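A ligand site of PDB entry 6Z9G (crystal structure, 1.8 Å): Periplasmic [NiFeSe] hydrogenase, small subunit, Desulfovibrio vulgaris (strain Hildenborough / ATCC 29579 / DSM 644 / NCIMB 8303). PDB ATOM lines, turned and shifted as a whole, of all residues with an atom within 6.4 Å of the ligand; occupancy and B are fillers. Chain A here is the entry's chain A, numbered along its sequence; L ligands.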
ATOM      1  N   ILE A 207      29.281 -22.193  12.579  1.00  0.00           N
ATOM      2  CA  ILE A 207      27.918 -21.680  12.394  1.00  0.00           C
ATOM      3  C   ILE A 207      27.952 -20.294  11.762  1.00  0.00           C
ATOM      4  O   ILE A 207      27.240 -20.019  10.779  1.00  0.00           O
ATOM      5  CB  ILE A 207      27.142 -21.672  13.734  1.00  0.00           C
ATOM      6  CG1 ILE A 207      26.779 -23.094  14.175  1.00  0.00           C
ATOM      7  CG2 ILE A 207      25.865 -20.811  13.615  1.00  0.00           C
ATOM      8  CD1 ILE A 207      26.029 -23.155  15.493  1.00  0.00           C
ATOM      9  N   HIS A 208      28.775 -19.396  12.296  1.00  0.00           N
ATOM     10  CA  HIS A 208      28.731 -18.002  11.859  1.00  0.00           C
ATOM     11  C   HIS A 208      29.077 -17.892  10.383  1.00  0.00           C
ATOM     12  O   HIS A 208      28.370 -17.242   9.617  1.00  0.00           O
ATOM     13  CB  HIS A 208      29.685 -17.170  12.725  1.00  0.00           C
ATOM     14  CG  HIS A 208      29.810 -15.745  12.276  1.00  0.00           C
ATOM     15  ND1 HIS A 208      28.844 -14.796  12.527  1.00  0.00           N
ATOM     16  CD2 HIS A 208      30.799 -15.105  11.600  1.00  0.00           C
ATOM     17  CE1 HIS A 208      29.235 -13.634  12.019  1.00  0.00           C
ATOM     18  NE2 HIS A 208      30.411 -13.801  11.457  1.00  0.00           N
ATOM     19  N   GLU A 209      30.167 -18.544   9.973  1.00  0.00           N
ATOM     20  CA  GLU A 209      30.588 -18.497   8.585  1.00  0.00           C
ATOM     21  C   GLU A 209      29.495 -18.990   7.651  1.00  0.00           C
ATOM     22  O   GLU A 209      29.562 -18.704   6.447  1.00  0.00           O
ATOM     23  CB  GLU A 209      31.862 -19.324   8.408  1.00  0.00           C
ATOM     24  CG  GLU A 209      33.066 -18.707   9.097  1.00  0.00           C
ATOM     25  CD  GLU A 209      34.251 -19.646   9.164  1.00  0.00           C
ATOM     26  OE1 GLU A 209      34.254 -20.670   8.449  1.00  0.00           O
ATOM     27  OE2 GLU A 209      35.188 -19.348   9.937  1.00  0.00           O
ATOM     28  N   CYS A 211      26.082 -18.601   8.607  1.00  0.00           N
ATOM     29  CA  CYS A 211      24.843 -18.107   9.156  1.00  0.00           C
ATOM     30  C   CYS A 211      24.089 -17.274   8.120  1.00  0.00           C
ATOM     31  O   CYS A 211      24.694 -16.451   7.439  1.00  0.00           O
ATOM     32  CB  CYS A 211      25.089 -17.257  10.397  1.00  0.00           C
ATOM     33  SG  CYS A 211      23.537 -16.722  11.146  1.00  0.00           S
ATOM     34  N   PRO A 212      22.763 -17.438   8.018  1.00  0.00           N
ATOM     35  CA  PRO A 212      21.992 -16.605   7.095  1.00  0.00           C
ATOM     36  C   PRO A 212      21.899 -15.131   7.491  1.00  0.00           C
ATOM     37  O   PRO A 212      21.426 -14.325   6.668  1.00  0.00           O
ATOM     38  CB  PRO A 212      20.606 -17.263   7.090  1.00  0.00           C
ATOM     39  CG  PRO A 212      20.542 -18.069   8.353  1.00  0.00           C
ATOM     40  CD  PRO A 212      21.949 -18.507   8.646  1.00  0.00           C
ATOM     41  N   TYR A 213      22.333 -14.750   8.688  1.00  0.00           N
ATOM     42  CA  TYR A 213      22.384 -13.347   9.093  1.00  0.00           C
ATOM     43  C   TYR A 213      23.783 -12.770   8.960  1.00  0.00           C
ATOM     44  O   TYR A 213      24.063 -11.680   9.474  1.00  0.00           O
ATOM     45  CB  TYR A 213      21.851 -13.170  10.523  1.00  0.00           C
ATOM     46  CG  TYR A 213      20.498 -13.793  10.708  1.00  0.00           C
ATOM     47  CD1 TYR A 213      19.384 -13.259  10.087  1.00  0.00           C
ATOM     48  CD2 TYR A 213      20.323 -14.926  11.489  1.00  0.00           C
ATOM     49  CE1 TYR A 213      18.146 -13.825  10.226  1.00  0.00           C
ATOM     50  CE2 TYR A 213      19.081 -15.501  11.638  1.00  0.00           C
ATOM     51  CZ  TYR A 213      17.992 -14.946  11.006  1.00  0.00           C
ATOM     52  OH  TYR A 213      16.740 -15.502  11.151  1.00  0.00           O
ATOM     53  N   LEU A 214      24.657 -13.473   8.234  1.00  0.00           N
ATOM     54  CA  LEU A 214      26.032 -13.018   8.077  1.00  0.00           C
ATOM     55  C   LEU A 214      26.096 -11.693   7.315  1.00  0.00           C
ATOM     56  O   LEU A 214      26.994 -10.884   7.575  1.00  0.00           O
ATOM     57  CB  LEU A 214      26.846 -14.086   7.352  1.00  0.00           C
ATOM     58  CG  LEU A 214      28.355 -13.842   7.252  1.00  0.00           C
ATOM     59  CD1 LEU A 214      28.944 -13.738   8.666  1.00  0.00           C
ATOM     60  CD2 LEU A 214      29.033 -14.941   6.443  1.00  0.00           C
ATOM     61  N   ASP A 215      25.165 -11.462   6.388  1.00  0.00           N
ATOM     62  CA  ASP A 215      25.108 -10.184   5.681  1.00  0.00           C
ATOM     63  C   ASP A 215      24.834  -9.035   6.660  1.00  0.00           C
ATOM     64  O   ASP A 215      25.491  -7.997   6.607  1.00  0.00           O
ATOM     65  CB  ASP A 215      24.027 -10.217   4.594  1.00  0.00           C
ATOM     66  CG  ASP A 215      22.651 -10.615   5.135  1.00  0.00           C
ATOM     67  OD1 ASP A 215      22.568 -11.296   6.172  1.00  0.00           O
ATOM     68  OD2 ASP A 215      21.633 -10.235   4.521  1.00  0.00           O
ATOM     69  N   LYS A 216      23.868  -9.228   7.550  1.00  0.00           N
ATOM     70  CA  LYS A 216      23.556  -8.191   8.533  1.00  0.00           C
ATOM     71  C   LYS A 216      24.734  -7.953   9.468  1.00  0.00           C
ATOM     72  O   LYS A 216      25.038  -6.814   9.818  1.00  0.00           O
ATOM     73  CB  LYS A 216      22.297  -8.567   9.323  1.00  0.00           C
ATOM     74  CG  LYS A 216      21.071  -8.837   8.454  1.00  0.00           C
ATOM     75  CD  LYS A 216      20.621  -7.566   7.746  1.00  0.00           C
ATOM     76  CE  LYS A 216      19.423  -7.805   6.856  1.00  0.00           C
ATOM     77  NZ  LYS A 216      19.057  -6.590   6.065  1.00  0.00           N
ATOM     78  N   TYR A 217      25.393  -9.033   9.900  1.00  0.00           N
ATOM     79  CA  TYR A 217      26.574  -8.907  10.747  1.00  0.00           C
ATOM     80  C   TYR A 217      27.629  -8.022  10.103  1.00  0.00           C
ATOM     81  O   TYR A 217      28.198  -7.139  10.765  1.00  0.00           O
ATOM     82  CB  TYR A 217      27.162 -10.295  11.022  1.00  0.00           C
ATOM     83  CG  TYR A 217      28.505 -10.261  11.721  1.00  0.00           C
ATOM     84  CD1 TYR A 217      28.595 -10.232  13.109  1.00  0.00           C
ATOM     85  CD2 TYR A 217      29.687 -10.240  10.990  1.00  0.00           C
ATOM     86  CE1 TYR A 217      29.833 -10.215  13.750  1.00  0.00           C
ATOM     87  CE2 TYR A 217      30.933 -10.213  11.613  1.00  0.00           C
ATOM     88  CZ  TYR A 217      30.993 -10.197  12.998  1.00  0.00           C
ATOM     89  OH  TYR A 217      32.220 -10.171  13.612  1.00  0.00           O
ATOM     90  N   MET A 222      22.419  -4.936  13.847  1.00  0.00           N
ATOM     91  CA  MET A 222      22.261  -5.801  15.011  1.00  0.00           C
ATOM     92  C   MET A 222      20.850  -5.689  15.566  1.00  0.00           C
ATOM     93  O   MET A 222      20.288  -4.595  15.627  1.00  0.00           O
ATOM     94  CB  MET A 222      23.256  -5.423  16.108  1.00  0.00           C
ATOM     95  CG  MET A 222      24.708  -5.468  15.694  1.00  0.00           C
ATOM     96  SD  MET A 222      25.212  -7.173  15.378  1.00  0.00           S
ATOM     97  CE  MET A 222      26.951  -6.938  14.987  1.00  0.00           C
ATOM     98  N   GLY A 231      17.912  -8.283  12.297  1.00  0.00           N
ATOM     99  CA  GLY A 231      19.311  -8.001  12.532  1.00  0.00           C
ATOM    100  C   GLY A 231      20.095  -9.213  12.952  1.00  0.00           C
ATOM    101  O   GLY A 231      19.554 -10.278  13.264  1.00  0.00           O
ATOM    102  N   CYS A 232      21.411  -9.031  12.951  1.00  0.00           N
ATOM    103  CA  CYS A 232      22.316 -10.042  13.483  1.00  0.00           C
ATOM    104  C   CYS A 232      22.181 -10.117  14.999  1.00  0.00           C
ATOM    105  O   CYS A 232      21.921  -9.112  15.676  1.00  0.00           O
ATOM    106  CB  CYS A 232      23.749  -9.738  13.076  1.00  0.00           C
ATOM    107  SG  CYS A 232      25.042 -10.606  13.969  1.00  0.00           S
ATOM    108  N   ARG A 233      22.351 -11.320  15.538  1.00  0.00           N
ATOM    109  CA  ARG A 233      22.161 -11.571  16.962  1.00  0.00           C
ATOM    110  C   ARG A 233      23.420 -11.349  17.790  1.00  0.00           C
ATOM    111  O   ARG A 233      23.421 -11.641  18.991  1.00  0.00           O
ATOM    112  CB  ARG A 233      21.649 -12.997  17.172  1.00  0.00           C
ATOM    113  CG  ARG A 233      20.177 -13.226  16.795  1.00  0.00           C
ATOM    114  CD  ARG A 233      19.862 -13.122  15.298  1.00  0.00           C
ATOM    115  NE  ARG A 233      18.634 -13.844  15.001  1.00  0.00           N
ATOM    116  CZ  ARG A 233      17.771 -13.539  14.029  1.00  0.00           C
ATOM    117  NH1 ARG A 233      17.979 -12.484  13.261  1.00  0.00           N
ATOM    118  NH2 ARG A 233      16.685 -14.289  13.861  1.00  0.00           N
ATOM    119  N   TYR A 234      24.478 -10.804  17.198  1.00  0.00           N
ATOM    120  CA  TYR A 234      25.770 -10.753  17.885  1.00  0.00           C
ATOM    121  C   TYR A 234      25.712  -9.944  19.175  1.00  0.00           C
ATOM    122  O   TYR A 234      26.266 -10.360  20.194  1.00  0.00           O
ATOM    123  CB  TYR A 234      26.848 -10.191  16.952  1.00  0.00           C
ATOM    124  CG  TYR A 234      28.189 -10.127  17.650  1.00  0.00           C
ATOM    125  CD1 TYR A 234      28.988 -11.242  17.750  1.00  0.00           C
ATOM    126  CD2 TYR A 234      28.644  -8.943  18.222  1.00  0.00           C
ATOM    127  CE1 TYR A 234      30.207 -11.207  18.382  1.00  0.00           C
ATOM    128  CE2 TYR A 234      29.870  -8.887  18.858  1.00  0.00           C
ATOM    129  CZ  TYR A 234      30.648 -10.024  18.937  1.00  0.00           C
ATOM    130  OH  TYR A 234      31.866  -9.979  19.569  1.00  0.00           O
ATOM    131  N   ASP A 235      25.091  -8.765  19.134  1.00  0.00           N
ATOM    132  CA  ASP A 235      25.059  -7.935  20.337  1.00  0.00           C
ATOM    133  C   ASP A 235      24.189  -8.550  21.429  1.00  0.00           C
ATOM    134  O   ASP A 235      24.424  -8.284  22.623  1.00  0.00           O
ATOM    135  CB  ASP A 235      24.574  -6.521  20.000  1.00  0.00           C
ATOM    136  CG  ASP A 235      25.677  -5.652  19.399  1.00  0.00           C
ATOM    137  OD1 ASP A 235      26.861  -6.039  19.495  1.00  0.00           O
ATOM    138  OD2 ASP A 235      25.368  -4.590  18.828  1.00  0.00           O
ATOM    139  N   CYS A 238      25.190 -13.755  20.703  1.00  0.00           N
ATOM    140  CA  CYS A 238      25.364 -14.930  19.854  1.00  0.00           C
ATOM    141  C   CYS A 238      26.819 -15.370  19.819  1.00  0.00           C
ATOM    142  O   CYS A 238      27.712 -14.571  19.528  1.00  0.00           O
ATOM    143  CB  CYS A 238      24.869 -14.646  18.432  1.00  0.00           C
ATOM    144  SG  CYS A 238      24.958 -16.112  17.333  1.00  0.00           S
ATOM    145  N   LYS A 239      27.068 -16.641  20.119  1.00  0.00           N
ATOM    146  CA  LYS A 239      28.394 -17.221  20.078  1.00  0.00           C
ATOM    147  C   LYS A 239      28.637 -18.027  18.817  1.00  0.00           C
ATOM    148  O   LYS A 239      29.603 -18.792  18.755  1.00  0.00           O
ATOM    149  CB  LYS A 239      28.639 -18.107  21.303  1.00  0.00           C
ATOM    150  CG  LYS A 239      28.461 -17.406  22.635  1.00  0.00           C
ATOM    151  CD  LYS A 239      29.245 -16.117  22.699  1.00  0.00           C
ATOM    152  CE  LYS A 239      29.168 -15.498  24.087  1.00  0.00           C
ATOM    153  NZ  LYS A 239      27.788 -15.108  24.429  1.00  0.00           N
ATOM    154  N   GLY A 240      27.771 -17.883  17.807  1.00  0.00           N
ATOM    155  CA  GLY A 240      27.969 -18.502  16.517  1.00  0.00           C
ATOM    156  C   GLY A 240      29.389 -18.351  15.993  1.00  0.00           C
ATOM    157  O   GLY A 240      29.975 -19.301  15.485  1.00  0.00           O
ATOM    158  N   PRO A 241      29.956 -17.137  16.089  1.00  0.00           N
ATOM    159  CA  PRO A 241      31.330 -16.959  15.589  1.00  0.00           C
ATOM    160  C   PRO A 241      32.361 -17.899  16.221  1.00  0.00           C
ATOM    161  O   PRO A 241      33.412 -18.117  15.603  1.00  0.00           O
ATOM    162  CB  PRO A 241      31.628 -15.479  15.919  1.00  0.00           C
ATOM    163  CG  PRO A 241      30.289 -14.813  15.780  1.00  0.00           C
ATOM    164  CD  PRO A 241      29.294 -15.845  16.338  1.00  0.00           C
ATOM    165  N   TRP A 258      15.868 -23.170  15.005  1.00  0.00           N
ATOM    166  CA  TRP A 258      17.185 -23.359  15.580  1.00  0.00           C
ATOM    167  C   TRP A 258      17.531 -22.129  16.410  1.00  0.00           C
ATOM    168  O   TRP A 258      16.834 -21.105  16.366  1.00  0.00           O
ATOM    169  CB  TRP A 258      18.232 -23.675  14.499  1.00  0.00           C
ATOM    170  CG  TRP A 258      18.577 -22.563  13.585  1.00  0.00           C
ATOM    171  CD1 TRP A 258      17.730 -21.884  12.735  1.00  0.00           C
ATOM    172  CD2 TRP A 258      19.876 -21.994  13.407  1.00  0.00           C
ATOM    173  NE1 TRP A 258      18.442 -20.923  12.060  1.00  0.00           N
ATOM    174  CE2 TRP A 258      19.755 -20.975  12.448  1.00  0.00           C
ATOM    175  CE3 TRP A 258      21.125 -22.238  13.973  1.00  0.00           C
ATOM    176  CZ2 TRP A 258      20.847 -20.214  12.038  1.00  0.00           C
ATOM    177  CZ3 TRP A 258      22.203 -21.478  13.568  1.00  0.00           C
ATOM    178  CH2 TRP A 258      22.061 -20.481  12.610  1.00  0.00           C
ATOM    179  N   VAL A 260      19.733 -19.675  16.664  1.00  0.00           N
ATOM    180  CA  VAL A 260      20.018 -18.319  16.210  1.00  0.00           C
ATOM    181  C   VAL A 260      18.764 -17.643  15.681  1.00  0.00           C
ATOM    182  O   VAL A 260      18.547 -16.442  15.909  1.00  0.00           O
ATOM    183  CB  VAL A 260      21.149 -18.338  15.159  1.00  0.00           C
ATOM    184  CG1 VAL A 260      21.409 -16.925  14.607  1.00  0.00           C
ATOM    185  CG2 VAL A 260      22.428 -18.920  15.766  1.00  0.00           C
ATOM    186  N   CYS A 265      22.742 -18.433  19.736  1.00  0.00           N
ATOM    187  CA  CYS A 265      23.565 -19.605  19.966  1.00  0.00           C
ATOM    188  C   CYS A 265      24.386 -19.397  21.234  1.00  0.00           C
ATOM    189  O   CYS A 265      24.933 -18.322  21.473  1.00  0.00           O
ATOM    190  CB  CYS A 265      24.471 -19.852  18.746  1.00  0.00           C
ATOM    191  SG  CYS A 265      25.681 -21.209  18.926  1.00  0.00           S
HETATM  192 FE1  LIG L   1      25.365 -15.023  15.307  1.00  0.00          FE
HETATM  193 FE2  LIG L   1      27.161 -14.698  13.398  1.00  0.00          FE
HETATM  194 FE3  LIG L   1      25.215 -12.855  13.674  1.00  0.00          FE
HETATM  195 FE4  LIG L   1      24.686 -15.394  12.643  1.00  0.00          FE
HETATM  196  S1  LIG L   1      25.951 -13.728  11.667  1.00  0.00           S
HETATM  197  S2  LIG L   1      23.475 -14.250  14.244  1.00  0.00           S
HETATM  198  S3  LIG L   1      26.111 -16.669  13.874  1.00  0.00           S
HETATM  199  S4  LIG L   1      26.868 -13.286  15.183  1.00  0.00           S
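ND1 of His 208 is bound to FE2 of the ligand. The side-chain sulfur (SG) of Cys 232 is bound to an iron atom (FE3) of the ligand (2.3 Å). SG of Cys 211 binds FE4 of the ligand (2.3 Å). The side-chain sulfur (SG) of Cys 238 is bound to an iron atom (FE1) of the ligand, at 2.3 Å. The backbone NH (N) of Arg 233 sits close to a sulfur (S2) of the ligand. The backbone NH of Leu 214 lies close to a sulfur (S1) of the ligand (3.7 Å).
O of Tyr 213 lies close to S1 of the ligand (3.5 Å). Residues that only touch the ligand: Tyr 217 (3.7 Å), Tyr 234 (3.6 Å), Gly 240 (3.7 Å), Pro 241 (3.7 Å) and Val 260 (3.4 Å). Hydrophobic or aromatic side chains within 4 Å of the ligand: His 208, Tyr 217, Tyr 234, Pro 241 and Val 260. Within 4 Å of the ligand: His 208, Cys 211, Tyr 213, Leu 214, Tyr 217, Cys 232, Arg 233, Tyr 234, Cys 238, Gly 240, Pro 241 and Val 260.
The backbone carbonyl oxygen (O) of Gly 240 is in hydrogen-bond range of the backbone NH (N) of His 208 (3.4 Å). The backbone NH of Tyr 234 sits close to the side-chain sulfur of Cys 232, at 3.3 Å. The side-chain sulfur of Cys 211 lies close to the backbone NH of Tyr 213, at 3.4 Å. The backbone carbonyl oxygen (O) of Arg 233 lies within hydrogen-bond range of the backbone NH (N) of Cys 238, at 3.2 Å. SG of Cys 238 lies close to N of Gly 240 (3.4 Å). The guanidinium group (NE) of Arg 233 lies within hydrogen-bond range of the backbone carbonyl oxygen (O) of Val 260 (2.8 Å). The guanidinium group (NH2) of Arg 233 lies within hydrogen-bond range of the side-chain hydroxyl (OH) of Tyr 213 (3.0 Å). NH1 of Arg 233 sits at hydrogen-bond distance from O of Gly 231, at 2.7 Å.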
